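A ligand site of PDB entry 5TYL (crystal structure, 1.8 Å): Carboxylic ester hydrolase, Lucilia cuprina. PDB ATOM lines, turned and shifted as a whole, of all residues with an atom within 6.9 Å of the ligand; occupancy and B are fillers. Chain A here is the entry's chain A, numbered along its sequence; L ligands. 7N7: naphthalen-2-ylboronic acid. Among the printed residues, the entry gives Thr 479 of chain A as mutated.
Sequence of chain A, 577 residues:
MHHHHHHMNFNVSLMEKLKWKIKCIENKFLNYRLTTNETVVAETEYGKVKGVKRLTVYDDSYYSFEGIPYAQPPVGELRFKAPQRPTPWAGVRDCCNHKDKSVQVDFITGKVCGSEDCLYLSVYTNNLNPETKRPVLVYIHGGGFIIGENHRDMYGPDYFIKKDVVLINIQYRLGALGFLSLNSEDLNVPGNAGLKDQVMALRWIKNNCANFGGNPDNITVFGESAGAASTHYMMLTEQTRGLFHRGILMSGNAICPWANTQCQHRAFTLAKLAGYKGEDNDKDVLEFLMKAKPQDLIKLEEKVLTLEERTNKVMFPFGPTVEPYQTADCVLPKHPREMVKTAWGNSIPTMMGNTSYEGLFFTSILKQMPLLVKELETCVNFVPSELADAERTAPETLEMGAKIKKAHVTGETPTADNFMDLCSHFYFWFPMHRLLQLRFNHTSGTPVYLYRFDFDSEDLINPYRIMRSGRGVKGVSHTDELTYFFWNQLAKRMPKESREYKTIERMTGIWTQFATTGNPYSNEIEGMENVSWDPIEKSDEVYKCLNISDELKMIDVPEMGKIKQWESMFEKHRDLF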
ATOM      1  N   HIS A 141      37.162 -27.803  -2.931  1.00  0.00           N
ATOM      2  CA  HIS A 141      36.625 -26.949  -3.970  1.00  0.00           C
ATOM      3  C   HIS A 141      35.145 -26.621  -3.729  1.00  0.00           C
ATOM      4  O   HIS A 141      34.408 -27.394  -3.101  1.00  0.00           O
ATOM      5  CB  HIS A 141      36.812 -27.589  -5.351  1.00  0.00           C
ATOM      6  CG  HIS A 141      35.973 -28.806  -5.585  1.00  0.00           C
ATOM      7  ND1 HIS A 141      34.650 -28.738  -5.950  1.00  0.00           N
ATOM      8  CD2 HIS A 141      36.270 -30.124  -5.482  1.00  0.00           C
ATOM      9  CE1 HIS A 141      34.157 -29.955  -6.086  1.00  0.00           C
ATOM     10  NE2 HIS A 141      35.123 -30.815  -5.813  1.00  0.00           N
ATOM     11  N   GLY A 142      34.732 -25.452  -4.203  1.00  0.00           N
ATOM     12  CA  GLY A 142      33.310 -25.102  -4.242  1.00  0.00           C
ATOM     13  C   GLY A 142      32.629 -25.609  -5.511  1.00  0.00           C
ATOM     14  O   GLY A 142      33.137 -26.489  -6.221  1.00  0.00           O
ATOM     15  N   GLY A 143      31.462 -25.045  -5.799  1.00  0.00           N
ATOM     16  CA  GLY A 143      30.659 -25.485  -6.923  1.00  0.00           C
ATOM     17  C   GLY A 143      29.234 -25.849  -6.532  1.00  0.00           C
ATOM     18  O   GLY A 143      28.573 -26.672  -7.187  1.00  0.00           O
ATOM     19  N   GLY A 144      28.751 -25.233  -5.457  1.00  0.00           N
ATOM     20  CA  GLY A 144      27.373 -25.442  -4.979  1.00  0.00           C
ATOM     21  C   GLY A 144      27.026 -26.860  -4.562  1.00  0.00           C
ATOM     22  O   GLY A 144      25.833 -27.210  -4.431  1.00  0.00           O
ATOM     23  N   PHE A 145      28.069 -27.658  -4.340  1.00  0.00           N
ATOM     24  CA  PHE A 145      27.957 -29.090  -4.041  1.00  0.00           C
ATOM     25  C   PHE A 145      27.397 -29.840  -5.267  1.00  0.00           C
ATOM     26  O   PHE A 145      26.998 -30.999  -5.139  1.00  0.00           O
ATOM     27  CB  PHE A 145      27.044 -29.378  -2.828  1.00  0.00           C
ATOM     28  CG  PHE A 145      27.496 -28.712  -1.547  1.00  0.00           C
ATOM     29  CD1 PHE A 145      28.475 -29.291  -0.761  1.00  0.00           C
ATOM     30  CD2 PHE A 145      26.886 -27.538  -1.119  1.00  0.00           C
ATOM     31  CE1 PHE A 145      28.882 -28.695   0.442  1.00  0.00           C
ATOM     32  CE2 PHE A 145      27.292 -26.913   0.082  1.00  0.00           C
ATOM     33  CZ  PHE A 145      28.296 -27.493   0.846  1.00  0.00           C
ATOM     34  N   ILE A 147      28.970 -28.979  -8.751  1.00  0.00           N
ATOM     35  CA  ILE A 147      30.038 -29.101  -9.721  1.00  0.00           C
ATOM     36  C   ILE A 147      31.373 -28.994  -9.013  1.00  0.00           C
ATOM     37  O   ILE A 147      31.433 -28.634  -7.820  1.00  0.00           O
ATOM     38  CB  ILE A 147      29.979 -28.042 -10.865  1.00  0.00           C
ATOM     39  CG1 ILE A 147      30.051 -26.615 -10.296  1.00  0.00           C
ATOM     40  CG2 ILE A 147      28.763 -28.232 -11.761  1.00  0.00           C
ATOM     41  CD1 ILE A 147      30.571 -25.582 -11.272  1.00  0.00           C
ATOM     42  N   GLU A 224      36.598 -22.507  -0.875  1.00  0.00           N
ATOM     43  CA  GLU A 224      35.843 -21.330  -1.301  1.00  0.00           C
ATOM     44  C   GLU A 224      34.402 -21.734  -1.689  1.00  0.00           C
ATOM     45  O   GLU A 224      34.211 -22.822  -2.225  1.00  0.00           O
ATOM     46  CB  GLU A 224      36.556 -20.663  -2.472  1.00  0.00           C
ATOM     47  CG  GLU A 224      35.940 -19.379  -2.955  1.00  0.00           C
ATOM     48  CD  GLU A 224      34.951 -19.610  -4.062  1.00  0.00           C
ATOM     49  OE1 GLU A 224      34.904 -20.743  -4.574  1.00  0.00           O
ATOM     50  OE2 GLU A 224      34.236 -18.663  -4.434  1.00  0.00           O
ATOM     51  N   SER A 225      33.417 -20.855  -1.460  1.00  0.00           N
ATOM     52  CA  SER A 225      32.013 -21.237  -1.698  1.00  0.00           C
ATOM     53  C   SER A 225      31.576 -22.477  -0.929  1.00  0.00           C
ATOM     54  O   SER A 225      31.695 -22.554   0.271  1.00  0.00           O
ATOM     55  CB  SER A 225      31.738 -21.477  -3.201  1.00  0.00           C
ATOM     56  OG  SER A 225      30.756 -20.663  -3.823  1.00  0.00           O
ATOM     57  N   ALA A 226      30.996 -23.429  -1.662  1.00  0.00           N
ATOM     58  CA  ALA A 226      30.588 -24.675  -1.035  1.00  0.00           C
ATOM     59  C   ALA A 226      31.780 -25.375  -0.376  1.00  0.00           C
ATOM     60  O   ALA A 226      31.590 -26.147   0.555  1.00  0.00           O
ATOM     61  CB  ALA A 226      29.904 -25.603  -2.064  1.00  0.00           C
ATOM     62  N   GLY A 227      32.997 -25.128  -0.865  1.00  0.00           N
ATOM     63  CA  GLY A 227      34.194 -25.570  -0.147  1.00  0.00           C
ATOM     64  C   GLY A 227      34.384 -24.880   1.200  1.00  0.00           C
ATOM     65  O   GLY A 227      34.932 -25.485   2.117  1.00  0.00           O
ATOM     66  N   ALA A 228      33.951 -23.631   1.330  1.00  0.00           N
ATOM     67  CA  ALA A 228      34.043 -22.905   2.602  1.00  0.00           C
ATOM     68  C   ALA A 228      32.985 -23.427   3.584  1.00  0.00           C
ATOM     69  O   ALA A 228      33.263 -23.729   4.748  1.00  0.00           O
ATOM     70  CB  ALA A 228      33.875 -21.426   2.382  1.00  0.00           C
ATOM     71  N   SER A 251      34.497 -16.934   1.405  1.00  0.00           N
ATOM     72  CA  SER A 251      33.176 -16.651   0.818  1.00  0.00           C
ATOM     73  C   SER A 251      32.152 -17.747   1.096  1.00  0.00           C
ATOM     74  O   SER A 251      31.493 -18.237   0.160  1.00  0.00           O
ATOM     75  CB  SER A 251      33.281 -16.457  -0.697  1.00  0.00           C
ATOM     76  OG  SER A 251      34.091 -15.372  -1.085  1.00  0.00           O
ATOM     77  N   TRP A 258      22.135 -21.134   1.297  1.00  0.00           N
ATOM     78  CA  TRP A 258      22.371 -22.091   0.194  1.00  0.00           C
ATOM     79  C   TRP A 258      23.183 -23.346   0.598  1.00  0.00           C
ATOM     80  O   TRP A 258      23.319 -24.289  -0.191  1.00  0.00           O
ATOM     81  CB  TRP A 258      23.103 -21.373  -0.949  1.00  0.00           C
ATOM     82  CG  TRP A 258      24.369 -20.622  -0.474  1.00  0.00           C
ATOM     83  CD1 TRP A 258      24.467 -19.296  -0.093  1.00  0.00           C
ATOM     84  CD2 TRP A 258      25.679 -21.181  -0.298  1.00  0.00           C
ATOM     85  NE1 TRP A 258      25.760 -19.010   0.290  1.00  0.00           N
ATOM     86  CE2 TRP A 258      26.522 -20.143   0.176  1.00  0.00           C
ATOM     87  CE3 TRP A 258      26.218 -22.473  -0.489  1.00  0.00           C
ATOM     88  CZ2 TRP A 258      27.882 -20.348   0.456  1.00  0.00           C
ATOM     89  CZ3 TRP A 258      27.572 -22.672  -0.229  1.00  0.00           C
ATOM     90  CH2 TRP A 258      28.388 -21.613   0.259  1.00  0.00           C
ATOM     91  N   MET A 315      18.405 -22.846  -3.535  1.00  0.00           N
ATOM     92  CA  MET A 315      19.253 -22.835  -4.732  1.00  0.00           C
ATOM     93  C   MET A 315      19.430 -24.224  -5.375  1.00  0.00           C
ATOM     94  O   MET A 315      19.466 -24.377  -6.588  1.00  0.00           O
ATOM     95  CB  MET A 315      20.628 -22.236  -4.379  1.00  0.00           C
ATOM     96  CG  MET A 315      20.539 -20.765  -3.955  1.00  0.00           C
ATOM     97  SD  MET A 315      19.893 -19.731  -5.298  1.00  0.00           S
ATOM     98  CE  MET A 315      18.503 -18.981  -4.464  1.00  0.00           C
ATOM     99  N   PHE A 316      19.539 -25.240  -4.532  1.00  0.00           N
ATOM    100  CA  PHE A 316      19.843 -26.566  -5.002  1.00  0.00           C
ATOM    101  C   PHE A 316      18.878 -27.565  -4.370  1.00  0.00           C
ATOM    102  O   PHE A 316      18.535 -27.443  -3.199  1.00  0.00           O
ATOM    103  CB  PHE A 316      21.283 -26.952  -4.677  1.00  0.00           C
ATOM    104  CG  PHE A 316      22.302 -25.918  -5.069  1.00  0.00           C
ATOM    105  CD1 PHE A 316      22.767 -25.846  -6.379  1.00  0.00           C
ATOM    106  CD2 PHE A 316      22.822 -25.056  -4.133  1.00  0.00           C
ATOM    107  CE1 PHE A 316      23.744 -24.890  -6.745  1.00  0.00           C
ATOM    108  CE2 PHE A 316      23.769 -24.101  -4.490  1.00  0.00           C
ATOM    109  CZ  PHE A 316      24.227 -24.021  -5.791  1.00  0.00           C
ATOM    110  N   PHE A 361      28.558 -11.972  -9.200  1.00  0.00           N
ATOM    111  CA  PHE A 361      28.578 -13.356  -9.674  1.00  0.00           C
ATOM    112  C   PHE A 361      27.247 -13.777 -10.312  1.00  0.00           C
ATOM    113  O   PHE A 361      27.172 -14.758 -11.040  1.00  0.00           O
ATOM    114  CB  PHE A 361      28.921 -14.219  -8.454  1.00  0.00           C
ATOM    115  CG  PHE A 361      29.027 -15.716  -8.695  1.00  0.00           C
ATOM    116  CD1 PHE A 361      30.143 -16.272  -9.328  1.00  0.00           C
ATOM    117  CD2 PHE A 361      28.036 -16.560  -8.205  1.00  0.00           C
ATOM    118  CE1 PHE A 361      30.242 -17.638  -9.486  1.00  0.00           C
ATOM    119  CE2 PHE A 361      28.129 -17.933  -8.384  1.00  0.00           C
ATOM    120  CZ  PHE A 361      29.233 -18.469  -9.021  1.00  0.00           C
ATOM    121  N   PHE A 362      26.204 -13.004 -10.036  1.00  0.00           N
ATOM    122  CA  PHE A 362      24.852 -13.378 -10.440  1.00  0.00           C
ATOM    123  C   PHE A 362      24.396 -12.712 -11.724  1.00  0.00           C
ATOM    124  O   PHE A 362      23.235 -12.840 -12.114  1.00  0.00           O
ATOM    125  CB  PHE A 362      23.862 -13.085  -9.319  1.00  0.00           C
ATOM    126  CG  PHE A 362      24.123 -13.893  -8.091  1.00  0.00           C
ATOM    127  CD1 PHE A 362      23.925 -15.258  -8.096  1.00  0.00           C
ATOM    128  CD2 PHE A 362      24.600 -13.290  -6.933  1.00  0.00           C
ATOM    129  CE1 PHE A 362      24.186 -16.022  -6.966  1.00  0.00           C
ATOM    130  CE2 PHE A 362      24.860 -14.054  -5.804  1.00  0.00           C
ATOM    131  CZ  PHE A 362      24.637 -15.414  -5.823  1.00  0.00           C
ATOM    132  N   ILE A 365      22.847 -15.023 -14.432  1.00  0.00           N
ATOM    133  CA  ILE A 365      21.521 -15.490 -14.029  1.00  0.00           C
ATOM    134  C   ILE A 365      20.518 -14.352 -14.113  1.00  0.00           C
ATOM    135  O   ILE A 365      19.389 -14.553 -14.569  1.00  0.00           O
ATOM    136  CB  ILE A 365      21.523 -16.105 -12.619  1.00  0.00           C
ATOM    137  CG1 ILE A 365      21.983 -17.563 -12.700  1.00  0.00           C
ATOM    138  CG2 ILE A 365      20.147 -16.038 -11.994  1.00  0.00           C
ATOM    139  CD1 ILE A 365      21.766 -18.353 -11.425  1.00  0.00           C
ATOM    140  N   TYR A 427      23.630 -13.940   0.641  1.00  0.00           N
ATOM    141  CA  TYR A 427      24.335 -15.191   0.477  1.00  0.00           C
ATOM    142  C   TYR A 427      25.662 -15.260   1.220  1.00  0.00           C
ATOM    143  O   TYR A 427      26.167 -16.368   1.453  1.00  0.00           O
ATOM    144  CB  TYR A 427      24.581 -15.466  -1.003  1.00  0.00           C
ATOM    145  CG  TYR A 427      23.314 -15.690  -1.830  1.00  0.00           C
ATOM    146  CD1 TYR A 427      22.490 -16.796  -1.585  1.00  0.00           C
ATOM    147  CD2 TYR A 427      22.978 -14.838  -2.866  1.00  0.00           C
ATOM    148  CE1 TYR A 427      21.341 -17.021  -2.337  1.00  0.00           C
ATOM    149  CE2 TYR A 427      21.845 -15.055  -3.631  1.00  0.00           C
ATOM    150  CZ  TYR A 427      21.039 -16.146  -3.363  1.00  0.00           C
ATOM    151  OH  TYR A 427      19.903 -16.341  -4.106  1.00  0.00           O
ATOM    152  N   PHE A 428      26.246 -14.120   1.606  1.00  0.00           N
ATOM    153  CA  PHE A 428      27.596 -14.178   2.156  1.00  0.00           C
ATOM    154  C   PHE A 428      27.860 -13.349   3.412  1.00  0.00           C
ATOM    155  O   PHE A 428      28.196 -13.896   4.453  1.00  0.00           O
ATOM    156  CB  PHE A 428      28.587 -13.769   1.060  1.00  0.00           C
ATOM    157  CG  PHE A 428      28.457 -14.588  -0.202  1.00  0.00           C
ATOM    158  CD1 PHE A 428      28.864 -15.916  -0.215  1.00  0.00           C
ATOM    159  CD2 PHE A 428      27.922 -14.051  -1.343  1.00  0.00           C
ATOM    160  CE1 PHE A 428      28.767 -16.686  -1.372  1.00  0.00           C
ATOM    161  CE2 PHE A 428      27.804 -14.829  -2.500  1.00  0.00           C
ATOM    162  CZ  PHE A 428      28.237 -16.135  -2.500  1.00  0.00           C
ATOM    163  N   TYR A 464      35.406 -19.472 -14.035  1.00  0.00           N
ATOM    164  CA  TYR A 464      34.152 -18.966 -13.475  1.00  0.00           C
ATOM    165  C   TYR A 464      33.726 -17.602 -14.016  1.00  0.00           C
ATOM    166  O   TYR A 464      32.542 -17.255 -13.966  1.00  0.00           O
ATOM    167  CB  TYR A 464      34.215 -18.851 -11.949  1.00  0.00           C
ATOM    168  CG  TYR A 464      34.279 -20.157 -11.224  1.00  0.00           C
ATOM    169  CD1 TYR A 464      33.206 -21.037 -11.262  1.00  0.00           C
ATOM    170  CD2 TYR A 464      35.392 -20.501 -10.471  1.00  0.00           C
ATOM    171  CE1 TYR A 464      33.257 -22.240 -10.575  1.00  0.00           C
ATOM    172  CE2 TYR A 464      35.460 -21.697  -9.797  1.00  0.00           C
ATOM    173  CZ  TYR A 464      34.382 -22.563  -9.850  1.00  0.00           C
ATOM    174  OH  TYR A 464      34.444 -23.759  -9.160  1.00  0.00           O
ATOM    175  N   MET A 467      31.663 -18.363 -16.905  1.00  0.00           N
ATOM    176  CA  MET A 467      30.364 -18.841 -16.451  1.00  0.00           C
ATOM    177  C   MET A 467      29.439 -17.703 -16.025  1.00  0.00           C
ATOM    178  O   MET A 467      28.246 -17.708 -16.346  1.00  0.00           O
ATOM    179  CB  MET A 467      30.531 -19.833 -15.293  1.00  0.00           C
ATOM    180  CG  MET A 467      29.221 -20.237 -14.639  1.00  0.00           C
ATOM    181  SD  MET A 467      29.380 -20.489 -12.855  1.00  0.00           S
ATOM    182  CE  MET A 467      29.825 -22.223 -12.796  1.00  0.00           C
ATOM    183  N   HIS A 478      32.372 -12.958  -6.464  1.00  0.00           N
ATOM    184  CA  HIS A 478      32.511 -14.341  -6.002  1.00  0.00           C
ATOM    185  C   HIS A 478      33.397 -15.139  -6.971  1.00  0.00           C
ATOM    186  O   HIS A 478      33.201 -15.058  -8.184  1.00  0.00           O
ATOM    187  CB  HIS A 478      31.120 -14.995  -5.910  1.00  0.00           C
ATOM    188  CG  HIS A 478      31.063 -16.259  -5.103  1.00  0.00           C
ATOM    189  ND1 HIS A 478      31.394 -16.295  -3.764  1.00  0.00           N
ATOM    190  CD2 HIS A 478      30.696 -17.511  -5.440  1.00  0.00           C
ATOM    191  CE1 HIS A 478      31.241 -17.530  -3.323  1.00  0.00           C
ATOM    192  NE2 HIS A 478      30.808 -18.286  -4.315  1.00  0.00           N
ATOM    193  N   THR A 479      34.356 -15.886  -6.420  1.00  0.00           N
ATOM    194  CA  THR A 479      35.378 -16.718  -7.125  1.00  0.00           C
ATOM    195  C   THR A 479      36.520 -15.944  -7.800  1.00  0.00           C
ATOM    196  O   THR A 479      37.469 -16.568  -8.301  1.00  0.00           O
ATOM    197  CB  THR A 479      34.788 -17.676  -8.256  1.00  0.00           C
ATOM    198  OG1 THR A 479      34.564 -16.958  -9.468  1.00  0.00           O
ATOM    199  CG2 THR A 479      33.512 -18.416  -7.801  1.00  0.00           C
HETATM  200  C13 7N7 L   1      26.511 -21.111  -6.538  1.00  0.00           C
HETATM  201  O01 7N7 L   1      30.762 -21.676  -6.186  1.00  0.00           O
HETATM  202  B02 7N7 L   1      29.958 -21.453  -4.742  1.00  0.00           B
HETATM  203  O03 7N7 L   1      29.889 -22.978  -4.050  1.00  0.00           O
HETATM  204  C05 7N7 L   1      28.381 -20.978  -5.036  1.00  0.00           C
HETATM  205  C06 7N7 L   1      27.667 -20.137  -4.154  1.00  0.00           C
HETATM  206  C07 7N7 L   1      26.312 -19.787  -4.511  1.00  0.00           C
HETATM  207  C08 7N7 L   1      25.548 -18.950  -3.687  1.00  0.00           C
HETATM  208  C09 7N7 L   1      24.247 -18.619  -4.038  1.00  0.00           C
HETATM  209  C10 7N7 L   1      23.678 -19.098  -5.219  1.00  0.00           C
HETATM  210  C11 7N7 L   1      24.435 -19.913  -6.034  1.00  0.00           C
HETATM  211  C12 7N7 L   1      25.759 -20.257  -5.675  1.00  0.00           C
HETATM  212  C14 7N7 L   1      27.810 -21.464  -6.223  1.00  0.00           C
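The backbone NH (N) of Ala 226 is in hydrogen-bond range of an oxygen (O03) of the ligand (2.7 Å). An oxygen (O03) of the ligand lies within hydrogen-bond range of the backbone NH (N) of Gly 143 (3.1 Å). O03 of the ligand sits at hydrogen-bond distance from N of Gly 144, 2.9 Å away. The side-chain hydroxyl of Ser 225 is bonded to a boron (B02) of the ligand (1.5 Å).
The backbone carbonyl oxygen (O) of Tyr 427 sits at hydrogen-bond distance from the indole nitrogen (NE1) of Trp 258 (2.9 Å). NE2 of His 478 lies within hydrogen-bond range of OG of Ser 225, at 2.4 Å. The side-chain carboxylate of Glu 224 lies close to a ring nitrogen (NE2) of His 478, at 3.5 Å. OH of Tyr 427 sits close to SD of Met 315.
Merely in contact with the ligand: Trp 258, Met 315, Phe 316, Phe 362, Tyr 427 and His 478. The nearest printed residue that does not touch the ligand is Phe 361 (4.02 Å).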
